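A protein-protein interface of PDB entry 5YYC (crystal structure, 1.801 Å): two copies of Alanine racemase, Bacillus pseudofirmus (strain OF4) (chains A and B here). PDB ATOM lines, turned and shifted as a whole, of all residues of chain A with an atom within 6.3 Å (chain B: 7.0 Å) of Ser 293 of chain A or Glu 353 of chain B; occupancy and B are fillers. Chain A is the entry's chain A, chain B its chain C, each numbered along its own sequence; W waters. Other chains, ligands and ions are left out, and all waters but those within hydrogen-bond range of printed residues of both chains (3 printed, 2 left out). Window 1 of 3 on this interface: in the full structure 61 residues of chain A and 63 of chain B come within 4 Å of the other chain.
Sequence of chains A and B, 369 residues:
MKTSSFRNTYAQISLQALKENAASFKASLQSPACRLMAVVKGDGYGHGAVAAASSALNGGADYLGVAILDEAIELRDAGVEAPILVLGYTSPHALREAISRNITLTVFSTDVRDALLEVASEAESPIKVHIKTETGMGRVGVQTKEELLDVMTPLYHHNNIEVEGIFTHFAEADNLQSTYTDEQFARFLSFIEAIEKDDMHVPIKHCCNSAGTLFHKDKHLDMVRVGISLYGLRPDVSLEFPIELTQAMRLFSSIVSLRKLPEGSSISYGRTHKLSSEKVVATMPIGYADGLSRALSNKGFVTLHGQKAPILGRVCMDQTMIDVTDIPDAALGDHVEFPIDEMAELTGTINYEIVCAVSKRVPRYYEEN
3 positions are printed for both chains. Of the 10 pairs that touch across the chains among the printed residues, none has its exchanged pair printed and touching as well.
Tyr 288 of chain A touches Ile 350 of chain B (OH to CD1, 3.9 Å). Tyr 352 of chain B touches Tyr 288 of chain A (CB to OH, 3.0 Å). Tyr 288 of chain A touches Glu 353 of chain B (CB to OE2, 3.7 Å). CA of Ser 293 of chain A touches OE2 of Glu 353 of chain B, at 3.8 Å. Arg 294 of chain A touches Gly 348 of chain B (NH1 to O, 3.8 Å). Thr 349 of chain B touches Arg 294 of chain A. Ile 350 of chain B touches Arg 294 of chain A. Tyr 352 of chain B touches Met 317 of chain A (CD2 to CE, 3.8 Å). Cys 356 of chain B touches Met 317 of chain A.
The side-chain sulfur (SG) of Cys 356 of chain B is in hydrogen-bond range of the backbone carbonyl oxygen (O) of Tyr 352 of chain B, at 3.4 Å. O of Arg 294 of chain A is in hydrogen-bond range of OG of Ser 297 of chain A. The side-chain hydroxyl (OG1) of Thr 349 of chain B lies within hydrogen-bond range of the side-chain carboxylate (OE1) of Glu 353 of chain B (2.6 Å). The backbone NH of Thr 349 of chain B lies within hydrogen-bond range of the backbone carbonyl oxygen of Ala 344 of chain B (2.8 Å). The backbone NH of Ala 295 of chain A sits close to the side-chain hydroxyl of Ser 293 of chain A. The backbone NH (N) of Tyr 288 of chain A lies within hydrogen-bond range of the backbone carbonyl oxygen (O) of Met 317 of chain A.
N of Arg 294 of chain A sits at hydrogen-bond distance from OE2 of Glu 353 of chain B (3.0 Å).
Of chain A, only Tyr 288, Ser 293 and Arg 294 come within 4 Å of Glu 353 of chain B. Printed residues of chain A within 4 Å of Ile 350 of chain B: Tyr 288 (3.9 Å) and Arg 294 (3.4 Å). Of the printed residues of chain B, Tyr 288 of chain A touches Ile 350, Tyr 352 and Glu 353. Of the printed residues of chain A, Tyr 352 of chain B touches Tyr 288 and Met 317. Of the printed residues of chain A, Thr 349 of chain B touches Arg 294 (3.6 Å). Of the printed residues of chain B, Met 317 of chain A touches Tyr 352 (3.8 Å) and Cys 356 (3.9 Å). Thr 347 of chain B touches none of the printed residues of chain A. The nearest printed residue of chain A that does not touch Gly 348 of chain B is Ala 295 of chain A (6.3 Å).
Water W3 bridges the side-chain carboxylate (OE1) of Glu 353 of chain B (2.7 Å) and the backbone NH (N) of Ala 295 of chain A (3.1 Å). Water W1 bridges the side-chain carboxylate of Glu 353 of chain B (2.9 Å) and the side-chain hydroxyl of Ser 293 of chain A (3.3 Å). Water W2 bridges NH1 of Arg 294 of chain A (3.1 Å) and O of Gly 348 of chain B (3.2 Å).
Of the 15 printed residues of chain B, 6 touch a printed residue of chain A. Hydrophobic or aromatic side chains of chain B within 4 Å of the printed part of chain A: Ile 350 and Tyr 352. Hydrophobic or aromatic side chains of chain A that line the printed part of chain B: Tyr 288 and Met 317. Among the printed residues, no Asp or Glu carboxylate lies within 4 Å of a Lys or Arg side-chain nitrogen of the other chain.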
ATOM      1  N   GLY A 287      -0.752   8.133  13.319  1.00  0.00           N
ATOM      2  CA  GLY A 287      -0.904   7.549  11.995  1.00  0.00           C
ATOM      3  C   GLY A 287      -1.849   8.385  11.161  1.00  0.00           C
ATOM      4  O   GLY A 287      -2.128   9.533  11.523  1.00  0.00           O
ATOM      5  N   TYR A 288      -2.359   7.838  10.058  1.00  0.00           N
ATOM      6  CA  TYR A 288      -3.084   8.696   9.128  1.00  0.00           C
ATOM      7  C   TYR A 288      -4.475   9.087   9.633  1.00  0.00           C
ATOM      8  O   TYR A 288      -5.063  10.056   9.129  1.00  0.00           O
ATOM      9  CB  TYR A 288      -3.156   8.066   7.715  1.00  0.00           C
ATOM     10  CG  TYR A 288      -3.733   6.669   7.631  1.00  0.00           C
ATOM     11  CD1 TYR A 288      -5.103   6.451   7.750  1.00  0.00           C
ATOM     12  CD2 TYR A 288      -2.907   5.574   7.374  1.00  0.00           C
ATOM     13  CE1 TYR A 288      -5.642   5.165   7.659  1.00  0.00           C
ATOM     14  CE2 TYR A 288      -3.436   4.292   7.285  1.00  0.00           C
ATOM     15  CZ  TYR A 288      -4.799   4.099   7.427  1.00  0.00           C
ATOM     16  OH  TYR A 288      -5.319   2.819   7.341  1.00  0.00           O
ATOM     17  N   GLY A 291      -4.061  12.370  10.717  1.00  0.00           N
ATOM     18  CA  GLY A 291      -3.743  13.291   9.641  1.00  0.00           C
ATOM     19  C   GLY A 291      -2.299  13.222   9.196  1.00  0.00           C
ATOM     20  O   GLY A 291      -1.862  14.022   8.372  1.00  0.00           O
ATOM     21  N   LEU A 292      -1.545  12.268   9.731  1.00  0.00           N
ATOM     22  CA  LEU A 292      -0.190  12.048   9.221  1.00  0.00           C
ATOM     23  C   LEU A 292      -0.305  11.359   7.869  1.00  0.00           C
ATOM     24  O   LEU A 292      -0.777  10.228   7.795  1.00  0.00           O
ATOM     25  CB  LEU A 292       0.638  11.202  10.196  1.00  0.00           C
ATOM     26  CG  LEU A 292       2.089  10.960   9.787  1.00  0.00           C
ATOM     27  CD1 LEU A 292       2.859  12.288   9.786  1.00  0.00           C
ATOM     28  CD2 LEU A 292       2.761   9.939  10.705  1.00  0.00           C
ATOM     29  N   SER A 293       0.110  12.030   6.797  1.00  0.00           N
ATOM     30  CA  SER A 293      -0.133  11.503   5.449  1.00  0.00           C
ATOM     31  C   SER A 293       0.468  10.117   5.227  1.00  0.00           C
ATOM     32  O   SER A 293       1.655   9.902   5.478  1.00  0.00           O
ATOM     33  CB  SER A 293       0.425  12.468   4.400  1.00  0.00           C
ATOM     34  OG  SER A 293       0.267  11.930   3.103  1.00  0.00           O
ATOM     35  N   ARG A 294      -0.337   9.177   4.741  1.00  0.00           N
ATOM     36  CA  ARG A 294       0.197   7.845   4.415  1.00  0.00           C
ATOM     37  C   ARG A 294       1.241   7.915   3.290  1.00  0.00           C
ATOM     38  O   ARG A 294       2.083   7.022   3.152  1.00  0.00           O
ATOM     39  CB  ARG A 294      -0.945   6.889   4.046  1.00  0.00           C
ATOM     40  CG  ARG A 294      -0.525   5.422   3.872  1.00  0.00           C
ATOM     41  CD  ARG A 294      -1.780   4.577   3.575  1.00  0.00           C
ATOM     42  NE  ARG A 294      -1.496   3.175   3.257  1.00  0.00           N
ATOM     43  CZ  ARG A 294      -1.225   2.710   2.040  1.00  0.00           C
ATOM     44  NH1 ARG A 294      -1.151   3.528   0.997  1.00  0.00           N
ATOM     45  NH2 ARG A 294      -1.008   1.412   1.869  1.00  0.00           N
ATOM     46  N   ALA A 295       1.222   8.993   2.508  1.00  0.00           N
ATOM     47  CA  ALA A 295       2.227   9.158   1.450  1.00  0.00           C
ATOM     48  C   ALA A 295       3.629   9.346   2.032  1.00  0.00           C
ATOM     49  O   ALA A 295       4.616   9.261   1.310  1.00  0.00           O
ATOM     50  CB  ALA A 295       1.866  10.324   0.534  1.00  0.00           C
ATOM     51  N   LEU A 296       3.725   9.575   3.341  1.00  0.00           N
ATOM     52  CA  LEU A 296       5.038   9.644   3.987  1.00  0.00           C
ATOM     53  C   LEU A 296       5.615   8.243   4.243  1.00  0.00           C
ATOM     54  O   LEU A 296       6.766   8.116   4.664  1.00  0.00           O
ATOM     55  CB  LEU A 296       4.946  10.430   5.309  1.00  0.00           C
ATOM     56  CG  LEU A 296       4.653  11.926   5.156  1.00  0.00           C
ATOM     57  CD1 LEU A 296       4.095  12.498   6.455  1.00  0.00           C
ATOM     58  CD2 LEU A 296       5.930  12.669   4.747  1.00  0.00           C
ATOM     59  N   SER A 297       4.829   7.199   3.973  1.00  0.00           N
ATOM     60  CA  SER A 297       5.331   5.814   4.066  1.00  0.00           C
ATOM     61  C   SER A 297       6.661   5.642   3.338  1.00  0.00           C
ATOM     62  O   SER A 297       6.791   6.002   2.163  1.00  0.00           O
ATOM     63  CB  SER A 297       4.315   4.814   3.483  1.00  0.00           C
ATOM     64  OG  SER A 297       3.095   4.826   4.221  1.00  0.00           O
ATOM     65  N   ILE A 311      10.969   7.342   8.556  1.00  0.00           N
ATOM     66  CA  ILE A 311       9.836   6.449   8.671  1.00  0.00           C
ATOM     67  C   ILE A 311      10.119   5.147   7.917  1.00  0.00           C
ATOM     68  O   ILE A 311      10.571   5.177   6.766  1.00  0.00           O
ATOM     69  CB  ILE A 311       8.563   7.133   8.128  1.00  0.00           C
ATOM     70  CG1 ILE A 311       8.168   8.283   9.057  1.00  0.00           C
ATOM     71  CG2 ILE A 311       7.422   6.138   7.985  1.00  0.00           C
ATOM     72  CD1 ILE A 311       7.032   9.150   8.536  1.00  0.00           C
ATOM     73  N   VAL A 315       2.912   3.886   7.011  1.00  0.00           N
ATOM     74  CA  VAL A 315       2.161   4.571   8.053  1.00  0.00           C
ATOM     75  C   VAL A 315       0.840   3.837   8.247  1.00  0.00           C
ATOM     76  O   VAL A 315       0.129   3.588   7.272  1.00  0.00           O
ATOM     77  CB  VAL A 315       1.892   6.046   7.664  1.00  0.00           C
ATOM     78  CG1 VAL A 315       0.955   6.726   8.672  1.00  0.00           C
ATOM     79  CG2 VAL A 315       3.212   6.826   7.510  1.00  0.00           C
ATOM     80  N   MET A 317      -3.006   3.387  10.491  1.00  0.00           N
ATOM     81  CA  MET A 317      -4.034   4.312  10.945  1.00  0.00           C
ATOM     82  C   MET A 317      -3.621   5.078  12.208  1.00  0.00           C
ATOM     83  O   MET A 317      -3.908   6.275  12.316  1.00  0.00           O
ATOM     84  CB  MET A 317      -5.366   3.566  11.184  1.00  0.00           C
ATOM     85  CG  MET A 317      -6.525   4.494  11.544  1.00  0.00           C
ATOM     86  SD  MET A 317      -8.194   3.758  11.552  1.00  0.00           S
ATOM     87  CE  MET A 317      -8.072   2.927   9.997  1.00  0.00           C
ATOM     88  N   MET A 343       7.113  17.776   5.241  1.00  0.00           N
ATOM     89  CA  MET A 343       6.075  16.774   4.966  1.00  0.00           C
ATOM     90  C   MET A 343       5.306  17.123   3.682  1.00  0.00           C
ATOM     91  O   MET A 343       4.968  16.240   2.898  1.00  0.00           O
ATOM     92  CB  MET A 343       5.102  16.636   6.138  1.00  0.00           C
ATOM     93  CG  MET A 343       5.683  15.850   7.317  1.00  0.00           C
ATOM     94  SD  MET A 343       4.433  15.524   8.580  1.00  0.00           S
ATOM     95  CE  MET A 343       4.113  17.170   9.229  1.00  0.00           C
ATOM     96  N   THR A 347       5.507  14.804   0.037  1.00  0.00           N
ATOM     97  CA  THR A 347       4.300  14.148  -0.449  1.00  0.00           C
ATOM     98  C   THR A 347       3.655  14.897  -1.610  1.00  0.00           C
ATOM     99  O   THR A 347       2.547  14.569  -2.024  1.00  0.00           O
ATOM    100  CB  THR A 347       3.258  13.963   0.662  1.00  0.00           C
ATOM    101  OG1 THR A 347       2.871  15.236   1.212  1.00  0.00           O
ATOM    102  CG2 THR A 347       3.825  13.055   1.766  1.00  0.00           C
ATOM    103  N   ILE A 354      -1.295  20.115   4.796  1.00  0.00           N
ATOM    104  CA  ILE A 354      -0.691  19.418   5.930  1.00  0.00           C
ATOM    105  C   ILE A 354      -1.308  19.878   7.250  1.00  0.00           C
ATOM    106  O   ILE A 354      -1.665  19.051   8.091  1.00  0.00           O
ATOM    107  CB  ILE A 354       0.850  19.624   5.977  1.00  0.00           C
ATOM    108  CG1 ILE A 354       1.521  19.020   4.734  1.00  0.00           C
ATOM    109  CG2 ILE A 354       1.454  19.028   7.283  1.00  0.00           C
ATOM    110  CD1 ILE A 354       1.275  17.512   4.544  1.00  0.00           C
ATOM    111  N   ILE B 228     -12.164  -2.425   8.684  1.00  0.00           N
ATOM    112  CA  ILE B 228     -12.536  -1.834   7.390  1.00  0.00           C
ATOM    113  C   ILE B 228     -13.783  -2.478   6.762  1.00  0.00           C
ATOM    114  O   ILE B 228     -14.635  -1.769   6.224  1.00  0.00           O
ATOM    115  CB  ILE B 228     -11.342  -1.893   6.378  1.00  0.00           C
ATOM    116  CG1 ILE B 228     -11.620  -1.029   5.126  1.00  0.00           C
ATOM    117  CG2 ILE B 228     -10.979  -3.344   5.993  1.00  0.00           C
ATOM    118  CD1 ILE B 228     -11.689   0.511   5.422  1.00  0.00           C
ATOM    119  N   GLY B 291     -11.209  17.265   3.641  1.00  0.00           N
ATOM    120  CA  GLY B 291     -10.598  15.959   3.506  1.00  0.00           C
ATOM    121  C   GLY B 291     -10.577  15.439   2.089  1.00  0.00           C
ATOM    122  O   GLY B 291     -10.178  14.304   1.855  1.00  0.00           O
ATOM    123  N   ALA B 344      -8.962   6.628  -3.680  1.00  0.00           N
ATOM    124  CA  ALA B 344      -7.778   5.988  -3.113  1.00  0.00           C
ATOM    125  C   ALA B 344      -6.813   5.557  -4.218  1.00  0.00           C
ATOM    126  O   ALA B 344      -5.616   5.874  -4.175  1.00  0.00           O
ATOM    127  CB  ALA B 344      -8.181   4.783  -2.252  1.00  0.00           C
ATOM    128  N   THR B 347      -4.947   8.387  -6.054  1.00  0.00           N
ATOM    129  CA  THR B 347      -3.960   9.128  -5.279  1.00  0.00           C
ATOM    130  C   THR B 347      -2.917   8.228  -4.615  1.00  0.00           C
ATOM    131  O   THR B 347      -2.122   8.693  -3.798  1.00  0.00           O
ATOM    132  CB  THR B 347      -4.622  10.008  -4.205  1.00  0.00           C
ATOM    133  OG1 THR B 347      -5.372   9.204  -3.276  1.00  0.00           O
ATOM    134  CG2 THR B 347      -5.541  11.046  -4.874  1.00  0.00           C
ATOM    135  N   GLY B 348      -2.928   6.951  -4.972  1.00  0.00           N
ATOM    136  CA  GLY B 348      -1.922   6.012  -4.508  1.00  0.00           C
ATOM    137  C   GLY B 348      -2.063   5.672  -3.037  1.00  0.00           C
ATOM    138  O   GLY B 348      -1.071   5.405  -2.359  1.00  0.00           O
ATOM    139  N   THR B 349      -3.295   5.675  -2.537  1.00  0.00           N
ATOM    140  CA  THR B 349      -3.521   5.291  -1.148  1.00  0.00           C
ATOM    141  C   THR B 349      -4.614   4.226  -1.050  1.00  0.00           C
ATOM    142  O   THR B 349      -4.875   3.491  -2.015  1.00  0.00           O
ATOM    143  CB  THR B 349      -3.849   6.530  -0.259  1.00  0.00           C
ATOM    144  OG1 THR B 349      -3.824   6.163   1.129  1.00  0.00           O
ATOM    145  CG2 THR B 349      -5.224   7.176  -0.611  1.00  0.00           C
ATOM    146  N   ILE B 350      -5.221   4.112   0.124  1.00  0.00           N
ATOM    147  CA  ILE B 350      -6.196   3.054   0.383  1.00  0.00           C
ATOM    148  C   ILE B 350      -7.482   3.644   0.931  1.00  0.00           C
ATOM    149  O   ILE B 350      -7.469   4.730   1.502  1.00  0.00           O
ATOM    150  CB  ILE B 350      -5.634   2.022   1.376  1.00  0.00           C
ATOM    151  CG1 ILE B 350      -5.128   2.735   2.630  1.00  0.00           C
ATOM    152  CG2 ILE B 350      -4.505   1.221   0.719  1.00  0.00           C
ATOM    153  CD1 ILE B 350      -4.549   1.776   3.698  1.00  0.00           C
ATOM    154  N   ASN B 351      -8.595   2.933   0.770  1.00  0.00           N
ATOM    155  CA  ASN B 351      -9.871   3.467   1.238  1.00  0.00           C
ATOM    156  C   ASN B 351      -9.866   3.838   2.733  1.00  0.00           C
ATOM    157  O   ASN B 351     -10.516   4.811   3.121  1.00  0.00           O
ATOM    158  CB  ASN B 351     -11.016   2.492   0.909  1.00  0.00           C
ATOM    159  CG  ASN B 351     -10.713   1.046   1.305  1.00  0.00           C
ATOM    160  OD1 ASN B 351      -9.883   0.781   2.169  1.00  0.00           O
ATOM    161  ND2 ASN B 351     -11.412   0.105   0.671  1.00  0.00           N
ATOM    162  N   TYR B 352      -9.112   3.103   3.560  1.00  0.00           N
ATOM    163  CA  TYR B 352      -8.972   3.451   4.977  1.00  0.00           C
ATOM    164  C   TYR B 352      -8.646   4.935   5.177  1.00  0.00           C
ATOM    165  O   TYR B 352      -9.241   5.609   6.013  1.00  0.00           O
ATOM    166  CB  TYR B 352      -7.839   2.689   5.669  1.00  0.00           C
ATOM    167  CG  TYR B 352      -7.869   1.177   5.762  1.00  0.00           C
ATOM    168  CD1 TYR B 352      -7.660   0.382   4.644  1.00  0.00           C
ATOM    169  CD2 TYR B 352      -7.974   0.550   7.007  1.00  0.00           C
ATOM    170  CE1 TYR B 352      -7.621  -1.020   4.750  1.00  0.00           C
ATOM    171  CE2 TYR B 352      -7.922  -0.840   7.125  1.00  0.00           C
ATOM    172  CZ  TYR B 352      -7.743  -1.610   5.998  1.00  0.00           C
ATOM    173  OH  TYR B 352      -7.699  -2.987   6.107  1.00  0.00           O
ATOM    174  N   GLU B 353      -7.640   5.415   4.451  1.00  0.00           N
ATOM    175  CA  GLU B 353      -7.211   6.797   4.641  1.00  0.00           C
ATOM    176  C   GLU B 353      -8.252   7.758   4.105  1.00  0.00           C
ATOM    177  O   GLU B 353      -8.517   8.794   4.726  1.00  0.00           O
ATOM    178  CB  GLU B 353      -5.866   7.075   3.975  1.00  0.00           C
ATOM    179  CG  GLU B 353      -5.346   8.482   4.331  1.00  0.00           C
ATOM    180  CD  GLU B 353      -4.002   8.819   3.716  1.00  0.00           C
ATOM    181  OE1 GLU B 353      -3.676   8.304   2.619  1.00  0.00           O
ATOM    182  OE2 GLU B 353      -3.267   9.631   4.335  1.00  0.00           O
ATOM    183  N   ILE B 354      -8.837   7.422   2.959  1.00  0.00           N
ATOM    184  CA  ILE B 354      -9.841   8.292   2.351  1.00  0.00           C
ATOM    185  C   ILE B 354     -10.996   8.552   3.320  1.00  0.00           C
ATOM    186  O   ILE B 354     -11.421   9.693   3.494  1.00  0.00           O
ATOM    187  CB  ILE B 354     -10.388   7.692   1.032  1.00  0.00           C
ATOM    188  CG1 ILE B 354      -9.272   7.588  -0.014  1.00  0.00           C
ATOM    189  CG2 ILE B 354     -11.577   8.522   0.491  1.00  0.00           C
ATOM    190  CD1 ILE B 354      -8.614   8.915  -0.382  1.00  0.00           C
ATOM    191  N   VAL B 355     -11.517   7.503   3.955  1.00  0.00           N
ATOM    192  CA  VAL B 355     -12.684   7.707   4.805  1.00  0.00           C
ATOM    193  C   VAL B 355     -12.310   8.374   6.137  1.00  0.00           C
ATOM    194  O   VAL B 355     -13.100   9.157   6.669  1.00  0.00           O
ATOM    195  CB  VAL B 355     -13.468   6.379   5.070  1.00  0.00           C
ATOM    196  CG1 VAL B 355     -14.080   5.856   3.773  1.00  0.00           C
ATOM    197  CG2 VAL B 355     -12.590   5.317   5.742  1.00  0.00           C
ATOM    198  N   CYS B 356     -11.122   8.083   6.673  1.00  0.00           N
ATOM    199  CA  CYS B 356     -10.673   8.758   7.895  1.00  0.00           C
ATOM    200  C   CYS B 356     -10.398  10.241   7.672  1.00  0.00           C
ATOM    201  O   CYS B 356     -10.532  11.048   8.596  1.00  0.00           O
ATOM    202  CB  CYS B 356      -9.404   8.113   8.450  1.00  0.00           C
ATOM    203  SG  CYS B 356      -9.724   6.521   9.221  1.00  0.00           S
ATOM    204  N   ALA B 357      -9.978  10.584   6.459  1.00  0.00           N
ATOM    205  CA  ALA B 357      -9.603  11.968   6.140  1.00  0.00           C
ATOM    206  C   ALA B 357     -10.808  12.909   6.016  1.00  0.00           C
ATOM    207  O   ALA B 357     -10.640  14.128   6.064  1.00  0.00           O
ATOM    208  CB  ALA B 357      -8.780  12.015   4.843  1.00  0.00           C
ATOM    209  N   VAL B 358     -12.013  12.367   5.836  1.00  0.00           N
ATOM    210  CA  VAL B 358     -13.194  13.232   5.747  1.00  0.00           C
ATOM    211  C   VAL B 358     -13.275  14.033   7.041  1.00  0.00           C
ATOM    212  O   VAL B 358     -13.410  13.468   8.116  1.00  0.00           O
ATOM    213  CB  VAL B 358     -14.488  12.428   5.504  1.00  0.00           C
ATOM    214  CG1 VAL B 358     -15.706  13.359   5.455  1.00  0.00           C
ATOM    215  CG2 VAL B 358     -14.357  11.631   4.201  1.00  0.00           C
HETATM  216  O   HOH W   1      -3.017  11.978   2.622  1.00  0.00           O
HETATM  217  O   HOH W   2      -0.287   6.447   0.522  1.00  0.00           O
HETATM  218  O   HOH W   3      -1.590   9.146   1.145  1.00  0.00           O
